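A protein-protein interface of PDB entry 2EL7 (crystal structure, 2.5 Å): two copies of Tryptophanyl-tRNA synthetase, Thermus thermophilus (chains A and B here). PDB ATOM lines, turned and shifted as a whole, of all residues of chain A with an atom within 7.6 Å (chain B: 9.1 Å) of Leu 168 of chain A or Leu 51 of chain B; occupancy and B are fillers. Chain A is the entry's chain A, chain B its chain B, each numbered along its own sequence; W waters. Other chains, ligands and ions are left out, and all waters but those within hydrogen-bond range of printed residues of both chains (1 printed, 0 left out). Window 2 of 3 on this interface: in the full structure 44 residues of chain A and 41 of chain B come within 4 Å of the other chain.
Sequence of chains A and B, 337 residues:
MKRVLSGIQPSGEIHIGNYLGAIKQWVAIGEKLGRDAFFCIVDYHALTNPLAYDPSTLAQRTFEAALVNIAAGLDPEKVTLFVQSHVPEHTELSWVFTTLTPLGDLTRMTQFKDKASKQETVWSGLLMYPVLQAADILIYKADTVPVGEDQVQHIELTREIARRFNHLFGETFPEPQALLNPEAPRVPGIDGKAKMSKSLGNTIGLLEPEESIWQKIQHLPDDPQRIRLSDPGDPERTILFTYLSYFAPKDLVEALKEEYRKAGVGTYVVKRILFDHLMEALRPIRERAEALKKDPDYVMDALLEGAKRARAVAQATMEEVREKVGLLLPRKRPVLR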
ATOM      1  N   THR A  99      26.516 -22.432  -3.743  1.00  0.00           N
ATOM      2  CA  THR A  99      25.385 -21.494  -3.854  1.00  0.00           C
ATOM      3  C   THR A  99      25.824 -20.031  -3.793  1.00  0.00           C
ATOM      4  O   THR A  99      25.087 -19.136  -4.221  1.00  0.00           O
ATOM      5  CB  THR A  99      24.283 -21.699  -2.737  1.00  0.00           C
ATOM      6  OG1 THR A  99      24.826 -21.386  -1.442  1.00  0.00           O
ATOM      7  CG2 THR A  99      23.752 -23.151  -2.723  1.00  0.00           C
ATOM      8  N   LEU A 100      27.021 -19.786  -3.266  1.00  0.00           N
ATOM      9  CA  LEU A 100      27.504 -18.414  -3.145  1.00  0.00           C
ATOM     10  C   LEU A 100      28.553 -18.064  -4.192  1.00  0.00           C
ATOM     11  O   LEU A 100      29.305 -17.116  -3.985  1.00  0.00           O
ATOM     12  CB  LEU A 100      28.121 -18.186  -1.767  1.00  0.00           C
ATOM     13  CG  LEU A 100      27.313 -18.506  -0.512  1.00  0.00           C
ATOM     14  CD1 LEU A 100      28.242 -18.432   0.694  1.00  0.00           C
ATOM     15  CD2 LEU A 100      26.156 -17.538  -0.378  1.00  0.00           C
ATOM     16  N   ILE A 161      34.972 -15.829  -1.911  1.00  0.00           N
ATOM     17  CA  ILE A 161      33.929 -16.601  -1.251  1.00  0.00           C
ATOM     18  C   ILE A 161      33.908 -16.320   0.246  1.00  0.00           C
ATOM     19  O   ILE A 161      32.848 -16.253   0.857  1.00  0.00           O
ATOM     20  CB  ILE A 161      34.123 -18.149  -1.507  1.00  0.00           C
ATOM     21  CG1 ILE A 161      33.825 -18.474  -2.979  1.00  0.00           C
ATOM     22  CG2 ILE A 161      33.201 -18.971  -0.613  1.00  0.00           C
ATOM     23  CD1 ILE A 161      34.084 -19.885  -3.345  1.00  0.00           C
ATOM     24  N   ALA A 162      35.078 -16.136   0.840  1.00  0.00           N
ATOM     25  CA  ALA A 162      35.136 -15.859   2.256  1.00  0.00           C
ATOM     26  C   ALA A 162      34.493 -14.511   2.533  1.00  0.00           C
ATOM     27  O   ALA A 162      33.683 -14.368   3.460  1.00  0.00           O
ATOM     28  CB  ALA A 162      36.568 -15.867   2.728  1.00  0.00           C
ATOM     29  N   ARG A 163      34.853 -13.514   1.730  1.00  0.00           N
ATOM     30  CA  ARG A 163      34.290 -12.187   1.905  1.00  0.00           C
ATOM     31  C   ARG A 163      32.785 -12.227   1.738  1.00  0.00           C
ATOM     32  O   ARG A 163      32.058 -11.654   2.555  1.00  0.00           O
ATOM     33  CB  ARG A 163      34.895 -11.190   0.913  1.00  0.00           C
ATOM     34  CG  ARG A 163      36.365 -10.867   1.190  1.00  0.00           C
ATOM     35  CD  ARG A 163      36.780  -9.555   0.541  1.00  0.00           C
ATOM     36  NE  ARG A 163      36.773  -9.643  -0.902  1.00  0.00           N
ATOM     37  CZ  ARG A 163      37.782 -10.131  -1.612  1.00  0.00           C
ATOM     38  NH1 ARG A 163      38.871 -10.560  -0.987  1.00  0.00           N
ATOM     39  NH2 ARG A 163      37.697 -10.205  -2.940  1.00  0.00           N
ATOM     40  N   ARG A 164      32.313 -12.920   0.705  1.00  0.00           N
ATOM     41  CA  ARG A 164      30.878 -13.000   0.464  1.00  0.00           C
ATOM     42  C   ARG A 164      30.177 -13.649   1.641  1.00  0.00           C
ATOM     43  O   ARG A 164      29.122 -13.174   2.068  1.00  0.00           O
ATOM     44  CB  ARG A 164      30.595 -13.780  -0.820  1.00  0.00           C
ATOM     45  CG  ARG A 164      29.175 -13.649  -1.300  1.00  0.00           C
ATOM     46  CD  ARG A 164      29.034 -14.172  -2.745  1.00  0.00           C
ATOM     47  NE  ARG A 164      29.798 -13.416  -3.751  1.00  0.00           N
ATOM     48  CZ  ARG A 164      30.841 -13.890  -4.429  1.00  0.00           C
ATOM     49  NH1 ARG A 164      31.458 -13.116  -5.322  1.00  0.00           N
ATOM     50  NH2 ARG A 164      31.275 -15.130  -4.215  1.00  0.00           N
ATOM     51  N   PHE A 165      30.778 -14.719   2.179  1.00  0.00           N
ATOM     52  CA  PHE A 165      30.208 -15.416   3.314  1.00  0.00           C
ATOM     53  C   PHE A 165      30.240 -14.529   4.551  1.00  0.00           C
ATOM     54  O   PHE A 165      29.221 -14.373   5.234  1.00  0.00           O
ATOM     55  CB  PHE A 165      30.964 -16.724   3.608  1.00  0.00           C
ATOM     56  CG  PHE A 165      30.298 -17.596   4.657  1.00  0.00           C
ATOM     57  CD1 PHE A 165      29.502 -18.688   4.281  1.00  0.00           C
ATOM     58  CD2 PHE A 165      30.434 -17.309   6.021  1.00  0.00           C
ATOM     59  CE1 PHE A 165      28.847 -19.480   5.247  1.00  0.00           C
ATOM     60  CE2 PHE A 165      29.787 -18.089   6.995  1.00  0.00           C
ATOM     61  CZ  PHE A 165      28.992 -19.176   6.605  1.00  0.00           C
ATOM     62  N   ASN A 166      31.400 -13.957   4.855  1.00  0.00           N
ATOM     63  CA  ASN A 166      31.519 -13.100   6.039  1.00  0.00           C
ATOM     64  C   ASN A 166      30.521 -11.935   6.055  1.00  0.00           C
ATOM     65  O   ASN A 166      29.937 -11.632   7.095  1.00  0.00           O
ATOM     66  CB  ASN A 166      32.944 -12.561   6.194  1.00  0.00           C
ATOM     67  CG  ASN A 166      33.960 -13.661   6.527  1.00  0.00           C
ATOM     68  OD1 ASN A 166      33.605 -14.745   7.013  1.00  0.00           O
ATOM     69  ND2 ASN A 166      35.233 -13.376   6.286  1.00  0.00           N
ATOM     70  N   HIS A 167      30.313 -11.303   4.904  1.00  0.00           N
ATOM     71  CA  HIS A 167      29.386 -10.190   4.812  1.00  0.00           C
ATOM     72  C   HIS A 167      27.932 -10.612   5.002  1.00  0.00           C
ATOM     73  O   HIS A 167      27.168  -9.913   5.686  1.00  0.00           O
ATOM     74  CB  HIS A 167      29.533  -9.476   3.453  1.00  0.00           C
ATOM     75  CG  HIS A 167      28.432  -8.495   3.162  1.00  0.00           C
ATOM     76  ND1 HIS A 167      28.246  -7.341   3.897  1.00  0.00           N
ATOM     77  CD2 HIS A 167      27.479  -8.483   2.196  1.00  0.00           C
ATOM     78  CE1 HIS A 167      27.231  -6.658   3.391  1.00  0.00           C
ATOM     79  NE2 HIS A 167      26.749  -7.328   2.357  1.00  0.00           N
ATOM     80  N   LEU A 168      27.548 -11.739   4.396  1.00  0.00           N
ATOM     81  CA  LEU A 168      26.171 -12.247   4.485  1.00  0.00           C
ATOM     82  C   LEU A 168      25.787 -12.953   5.791  1.00  0.00           C
ATOM     83  O   LEU A 168      24.627 -12.946   6.161  1.00  0.00           O
ATOM     84  CB  LEU A 168      25.883 -13.249   3.353  1.00  0.00           C
ATOM     85  CG  LEU A 168      26.074 -12.905   1.879  1.00  0.00           C
ATOM     86  CD1 LEU A 168      25.936 -14.189   1.041  1.00  0.00           C
ATOM     87  CD2 LEU A 168      25.045 -11.856   1.453  1.00  0.00           C
ATOM     88  N   PHE A 169      26.729 -13.597   6.477  1.00  0.00           N
ATOM     89  CA  PHE A 169      26.334 -14.310   7.679  1.00  0.00           C
ATOM     90  C   PHE A 169      27.062 -13.977   8.961  1.00  0.00           C
ATOM     91  O   PHE A 169      26.735 -14.555   9.989  1.00  0.00           O
ATOM     92  CB  PHE A 169      26.428 -15.832   7.449  1.00  0.00           C
ATOM     93  CG  PHE A 169      25.813 -16.295   6.153  1.00  0.00           C
ATOM     94  CD1 PHE A 169      26.624 -16.716   5.090  1.00  0.00           C
ATOM     95  CD2 PHE A 169      24.423 -16.310   5.985  1.00  0.00           C
ATOM     96  CE1 PHE A 169      26.066 -17.147   3.884  1.00  0.00           C
ATOM     97  CE2 PHE A 169      23.849 -16.736   4.780  1.00  0.00           C
ATOM     98  CZ  PHE A 169      24.667 -17.156   3.727  1.00  0.00           C
ATOM     99  N   GLY A 170      28.017 -13.055   8.922  1.00  0.00           N
ATOM    100  CA  GLY A 170      28.778 -12.728  10.120  1.00  0.00           C
ATOM    101  C   GLY A 170      30.205 -13.222   9.920  1.00  0.00           C
ATOM    102  O   GLY A 170      30.398 -14.283   9.317  1.00  0.00           O
ATOM    103  N   GLU A 171      31.202 -12.485  10.413  1.00  0.00           N
ATOM    104  CA  GLU A 171      32.605 -12.859  10.214  1.00  0.00           C
ATOM    105  C   GLU A 171      32.853 -14.311  10.580  1.00  0.00           C
ATOM    106  O   GLU A 171      32.658 -14.717  11.720  1.00  0.00           O
ATOM    107  CB  GLU A 171      33.556 -11.953  11.022  1.00  0.00           C
ATOM    108  CG  GLU A 171      35.034 -12.140  10.602  1.00  0.00           C
ATOM    109  CD  GLU A 171      36.026 -11.277  11.373  1.00  0.00           C
ATOM    110  OE1 GLU A 171      36.091 -11.426  12.610  1.00  0.00           O
ATOM    111  OE2 GLU A 171      36.752 -10.464  10.737  1.00  0.00           O
ATOM    112  N   LYS A 324      24.834 -20.250  11.267  1.00  0.00           N
ATOM    113  CA  LYS A 324      24.823 -18.926  10.653  1.00  0.00           C
ATOM    114  C   LYS A 324      24.034 -18.869   9.355  1.00  0.00           C
ATOM    115  O   LYS A 324      23.496 -17.838   8.991  1.00  0.00           O
ATOM    116  CB  LYS A 324      26.254 -18.438  10.411  1.00  0.00           C
ATOM    117  CG  LYS A 324      27.013 -18.085  11.700  1.00  0.00           C
ATOM    118  CD  LYS A 324      28.340 -17.386  11.417  1.00  0.00           C
ATOM    119  CE  LYS A 324      29.042 -17.024  12.706  1.00  0.00           C
ATOM    120  NZ  LYS A 324      30.497 -16.801  12.500  1.00  0.00           N
ATOM    121  N   VAL A 325      23.978 -19.990   8.656  1.00  0.00           N
ATOM    122  CA  VAL A 325      23.245 -20.106   7.399  1.00  0.00           C
ATOM    123  C   VAL A 325      21.755 -20.224   7.754  1.00  0.00           C
ATOM    124  O   VAL A 325      20.883 -20.118   6.896  1.00  0.00           O
ATOM    125  CB  VAL A 325      23.789 -21.355   6.629  1.00  0.00           C
ATOM    126  CG1 VAL A 325      22.676 -22.169   6.018  1.00  0.00           C
ATOM    127  CG2 VAL A 325      24.802 -20.896   5.592  1.00  0.00           C
ATOM    128  N   ALA B  46      16.740 -24.040  -0.285  1.00  0.00           N
ATOM    129  CA  ALA B  46      16.489 -22.632   0.021  1.00  0.00           C
ATOM    130  C   ALA B  46      17.665 -21.751  -0.373  1.00  0.00           C
ATOM    131  O   ALA B  46      17.464 -20.626  -0.829  1.00  0.00           O
ATOM    132  CB  ALA B  46      16.187 -22.452   1.512  1.00  0.00           C
ATOM    133  N   LEU B  47      18.884 -22.269  -0.210  1.00  0.00           N
ATOM    134  CA  LEU B  47      20.095 -21.507  -0.506  1.00  0.00           C
ATOM    135  C   LEU B  47      20.409 -21.168  -1.979  1.00  0.00           C
ATOM    136  O   LEU B  47      21.214 -20.269  -2.245  1.00  0.00           O
ATOM    137  CB  LEU B  47      21.323 -22.200   0.115  1.00  0.00           C
ATOM    138  CG  LEU B  47      21.326 -22.634   1.595  1.00  0.00           C
ATOM    139  CD1 LEU B  47      22.747 -22.586   2.110  1.00  0.00           C
ATOM    140  CD2 LEU B  47      20.477 -21.741   2.455  1.00  0.00           C
ATOM    141  N   THR B  48      19.784 -21.849  -2.936  1.00  0.00           N
ATOM    142  CA  THR B  48      20.093 -21.564  -4.331  1.00  0.00           C
ATOM    143  C   THR B  48      19.911 -20.090  -4.727  1.00  0.00           C
ATOM    144  O   THR B  48      20.468 -19.644  -5.744  1.00  0.00           O
ATOM    145  CB  THR B  48      19.298 -22.474  -5.258  1.00  0.00           C
ATOM    146  OG1 THR B  48      17.897 -22.307  -5.027  1.00  0.00           O
ATOM    147  CG2 THR B  48      19.684 -23.930  -4.992  1.00  0.00           C
ATOM    148  N   ASN B  49      19.129 -19.341  -3.941  1.00  0.00           N
ATOM    149  CA  ASN B  49      18.941 -17.892  -4.159  1.00  0.00           C
ATOM    150  C   ASN B  49      19.597 -17.203  -2.945  1.00  0.00           C
ATOM    151  O   ASN B  49      18.923 -16.747  -2.018  1.00  0.00           O
ATOM    152  CB  ASN B  49      17.461 -17.528  -4.255  1.00  0.00           C
ATOM    153  CG  ASN B  49      16.801 -18.146  -5.475  1.00  0.00           C
ATOM    154  OD1 ASN B  49      16.039 -19.103  -5.360  1.00  0.00           O
ATOM    155  ND2 ASN B  49      17.111 -17.610  -6.657  1.00  0.00           N
ATOM    156  N   PRO B  50      20.938 -17.104  -2.973  1.00  0.00           N
ATOM    157  CA  PRO B  50      21.844 -16.534  -1.978  1.00  0.00           C
ATOM    158  C   PRO B  50      21.383 -15.256  -1.300  1.00  0.00           C
ATOM    159  O   PRO B  50      21.441 -15.138  -0.076  1.00  0.00           O
ATOM    160  CB  PRO B  50      23.138 -16.307  -2.767  1.00  0.00           C
ATOM    161  CG  PRO B  50      23.021 -17.211  -3.929  1.00  0.00           C
ATOM    162  CD  PRO B  50      21.596 -17.123  -4.292  1.00  0.00           C
ATOM    163  N   LEU B  51      20.936 -14.293  -2.093  1.00  0.00           N
ATOM    164  CA  LEU B  51      20.521 -13.019  -1.529  1.00  0.00           C
ATOM    165  C   LEU B  51      19.034 -12.911  -1.141  1.00  0.00           C
ATOM    166  O   LEU B  51      18.711 -12.295  -0.129  1.00  0.00           O
ATOM    167  CB  LEU B  51      20.924 -11.887  -2.497  1.00  0.00           C
ATOM    168  CG  LEU B  51      22.334 -11.998  -3.125  1.00  0.00           C
ATOM    169  CD1 LEU B  51      22.508 -10.948  -4.219  1.00  0.00           C
ATOM    170  CD2 LEU B  51      23.412 -11.860  -2.064  1.00  0.00           C
ATOM    171  N   ALA B  52      18.145 -13.533  -1.912  1.00  0.00           N
ATOM    172  CA  ALA B  52      16.706 -13.465  -1.647  1.00  0.00           C
ATOM    173  C   ALA B  52      16.159 -14.327  -0.503  1.00  0.00           C
ATOM    174  O   ALA B  52      15.149 -13.969   0.113  1.00  0.00           O
ATOM    175  CB  ALA B  52      15.942 -13.779  -2.918  1.00  0.00           C
ATOM    176  N   TYR B  53      16.790 -15.467  -0.226  1.00  0.00           N
ATOM    177  CA  TYR B  53      16.312 -16.341   0.851  1.00  0.00           C
ATOM    178  C   TYR B  53      16.611 -15.627   2.178  1.00  0.00           C
ATOM    179  O   TYR B  53      17.346 -14.631   2.187  1.00  0.00           O
ATOM    180  CB  TYR B  53      16.993 -17.718   0.725  1.00  0.00           C
ATOM    181  CG  TYR B  53      18.123 -18.005   1.681  1.00  0.00           C
ATOM    182  CD1 TYR B  53      17.875 -18.608   2.910  1.00  0.00           C
ATOM    183  CD2 TYR B  53      19.442 -17.716   1.340  1.00  0.00           C
ATOM    184  CE1 TYR B  53      18.903 -18.921   3.776  1.00  0.00           C
ATOM    185  CE2 TYR B  53      20.488 -18.028   2.200  1.00  0.00           C
ATOM    186  CZ  TYR B  53      20.213 -18.633   3.424  1.00  0.00           C
ATOM    187  OH  TYR B  53      21.233 -18.956   4.295  1.00  0.00           O
ATOM    188  N   ASP B  54      16.050 -16.091   3.291  1.00  0.00           N
ATOM    189  CA  ASP B  54      16.266 -15.392   4.560  1.00  0.00           C
ATOM    190  C   ASP B  54      16.755 -16.319   5.679  1.00  0.00           C
ATOM    191  O   ASP B  54      15.977 -17.048   6.297  1.00  0.00           O
ATOM    192  CB  ASP B  54      14.957 -14.682   4.964  1.00  0.00           C
ATOM    193  CG  ASP B  54      15.083 -13.863   6.256  1.00  0.00           C
ATOM    194  OD1 ASP B  54      14.022 -13.484   6.797  1.00  0.00           O
ATOM    195  OD2 ASP B  54      16.217 -13.589   6.732  1.00  0.00           O
ATOM    196  N   PRO B  55      18.064 -16.272   5.974  1.00  0.00           N
ATOM    197  CA  PRO B  55      18.693 -17.100   7.013  1.00  0.00           C
ATOM    198  C   PRO B  55      18.007 -17.021   8.373  1.00  0.00           C
ATOM    199  O   PRO B  55      17.992 -17.998   9.129  1.00  0.00           O
ATOM    200  CB  PRO B  55      20.125 -16.560   7.075  1.00  0.00           C
ATOM    201  CG  PRO B  55      20.336 -15.976   5.706  1.00  0.00           C
ATOM    202  CD  PRO B  55      19.032 -15.310   5.405  1.00  0.00           C
ATOM    203  N   SER B  56      17.444 -15.863   8.689  1.00  0.00           N
ATOM    204  CA  SER B  56      16.795 -15.683   9.981  1.00  0.00           C
ATOM    205  C   SER B  56      15.485 -16.444  10.150  1.00  0.00           C
ATOM    206  O   SER B  56      15.013 -16.598  11.258  1.00  0.00           O
ATOM    207  CB  SER B  56      16.587 -14.181  10.273  1.00  0.00           C
ATOM    208  OG  SER B  56      15.974 -13.511   9.182  1.00  0.00           O
ATOM    209  N   GLN B 119      17.749 -13.338 -14.131  1.00  0.00           N
ATOM    210  CA  GLN B 119      18.741 -13.023 -13.096  1.00  0.00           C
ATOM    211  C   GLN B 119      19.955 -12.250 -13.608  1.00  0.00           C
ATOM    212  O   GLN B 119      20.507 -12.567 -14.666  1.00  0.00           O
ATOM    213  CB  GLN B 119      19.232 -14.305 -12.423  1.00  0.00           C
ATOM    214  CG  GLN B 119      18.150 -15.113 -11.749  1.00  0.00           C
ATOM    215  CD  GLN B 119      18.692 -16.011 -10.654  1.00  0.00           C
ATOM    216  OE1 GLN B 119      17.956 -16.816 -10.071  1.00  0.00           O
ATOM    217  NE2 GLN B 119      19.984 -15.875 -10.359  1.00  0.00           N
ATOM    218  N   GLU B 120      20.375 -11.244 -12.845  1.00  0.00           N
ATOM    219  CA  GLU B 120      21.532 -10.432 -13.222  1.00  0.00           C
ATOM    220  C   GLU B 120      22.831 -11.097 -12.758  1.00  0.00           C
ATOM    221  O   GLU B 120      23.930 -10.615 -13.032  1.00  0.00           O
ATOM    222  CB  GLU B 120      21.411  -9.016 -12.641  1.00  0.00           C
ATOM    223  CG  GLU B 120      22.490  -8.023 -13.121  1.00  0.00           C
ATOM    224  CD  GLU B 120      22.745  -8.060 -14.641  1.00  0.00           C
ATOM    225  OE1 GLU B 120      23.523  -8.930 -15.099  1.00  0.00           O
ATOM    226  OE2 GLU B 120      22.170  -7.219 -15.379  1.00  0.00           O
ATOM    227  N   THR B 121      22.698 -12.202 -12.033  1.00  0.00           N
ATOM    228  CA  THR B 121      23.855 -12.967 -11.590  1.00  0.00           C
ATOM    229  C   THR B 121      23.443 -14.412 -11.527  1.00  0.00           C
ATOM    230  O   THR B 121      22.536 -14.777 -10.777  1.00  0.00           O
ATOM    231  CB  THR B 121      24.360 -12.574 -10.206  1.00  0.00           C
ATOM    232  OG1 THR B 121      24.892 -11.246 -10.248  1.00  0.00           O
ATOM    233  CG2 THR B 121      25.458 -13.546  -9.764  1.00  0.00           C
ATOM    234  N   TRP B 123      23.960 -17.678 -10.132  1.00  0.00           N
ATOM    235  CA  TRP B 123      24.665 -18.371  -9.065  1.00  0.00           C
ATOM    236  C   TRP B 123      24.741 -19.855  -9.411  1.00  0.00           C
ATOM    237  O   TRP B 123      23.777 -20.427  -9.926  1.00  0.00           O
ATOM    238  CB  TRP B 123      23.964 -18.168  -7.723  1.00  0.00           C
ATOM    239  CG  TRP B 123      23.787 -16.724  -7.360  1.00  0.00           C
ATOM    240  CD1 TRP B 123      22.692 -15.940  -7.616  1.00  0.00           C
ATOM    241  CD2 TRP B 123      24.761 -15.863  -6.744  1.00  0.00           C
ATOM    242  NE1 TRP B 123      22.931 -14.652  -7.204  1.00  0.00           N
ATOM    243  CE2 TRP B 123      24.190 -14.575  -6.667  1.00  0.00           C
ATOM    244  CE3 TRP B 123      26.065 -16.056  -6.253  1.00  0.00           C
ATOM    245  CZ2 TRP B 123      24.875 -13.479  -6.122  1.00  0.00           C
ATOM    246  CZ3 TRP B 123      26.746 -14.968  -5.709  1.00  0.00           C
ATOM    247  CH2 TRP B 123      26.146 -13.693  -5.651  1.00  0.00           C
HETATM  248  O   HOH W   1      23.165 -20.591  -5.789  1.00  0.00           O
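O of Val 325 of chain A is in hydrogen-bond range of OH of Tyr 53 of chain B (2.9 Å).
NH2 of Arg 164 of chain A lies within hydrogen-bond range of O of Leu 100 of chain A (2.8 Å).
Among the printed residues, merely in contact across the chains: Thr 99 of chain A with Pro 50 of chain B (2.8 Å), Thr 99 of chain A with Leu 47 of chain B (3.4 Å), Phe 169 of chain A with Tyr 53 of chain B (3.5 Å), Val 325 of chain A with Pro 55 of chain B (3.6 Å), Phe 169 of chain A with Pro 55 of chain B (3.7 Å), Leu 100 of chain A with Trp 123 of chain B (3.8 Å), Thr 99 of chain A with Trp 123 of chain B (3.8 Å), Arg 164 of chain A with Trp 123 of chain B (3.8 Å), Leu 168 of chain A with Leu 51 of chain B (3.9 Å) and Val 325 of chain A with Leu 47 of chain B (3.9 Å).
Printed residues of chain B within 4 Å of Thr 99 of chain A: Leu 47, Pro 50 and Trp 123.
Of the printed residues of chain B, Leu 100 of chain A touches Trp 123.
Of chain B, only Leu 51 comes within 4 Å of Leu 168 of chain A.
Phe 169 of chain A touches just these residues of chain B: Tyr 53 (3.5 Å) and Pro 55 (3.7 Å).
Of the printed residues of chain B, Val 325 of chain A touches Leu 47, Tyr 53 and Pro 55.
Printed residues of chain A within 4 Å of Leu 47 of chain B: Thr 99 and Val 325.
Of chain A, only Leu 168 (3.9 Å) comes within 4 Å of Leu 51 of chain B.
Of the printed residues of chain A, Pro 55 of chain B touches Phe 169 (3.7 Å) and Val 325 (3.6 Å).
The nearest residue of chain B that does not touch Leu 168 of chain A is Pro 50 of chain B (4.7 Å).
The nearest printed residue of chain A that does not touch Trp 123 of chain B is Leu 168 of chain A (6.7 Å).
Among the printed residues, no Asp or Glu carboxylate lies within 4 Å of a Lys or Arg side-chain nitrogen of the other chain.
No position is printed for both chains.
Of the 11 pairs that touch across the chains among the printed residues, none has its exchanged pair printed and touching as well.
Water W1 lies within hydrogen-bond range of O of Thr 48 of chain B (2.9 Å) and O of Thr 99 of chain A (2.9 Å).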
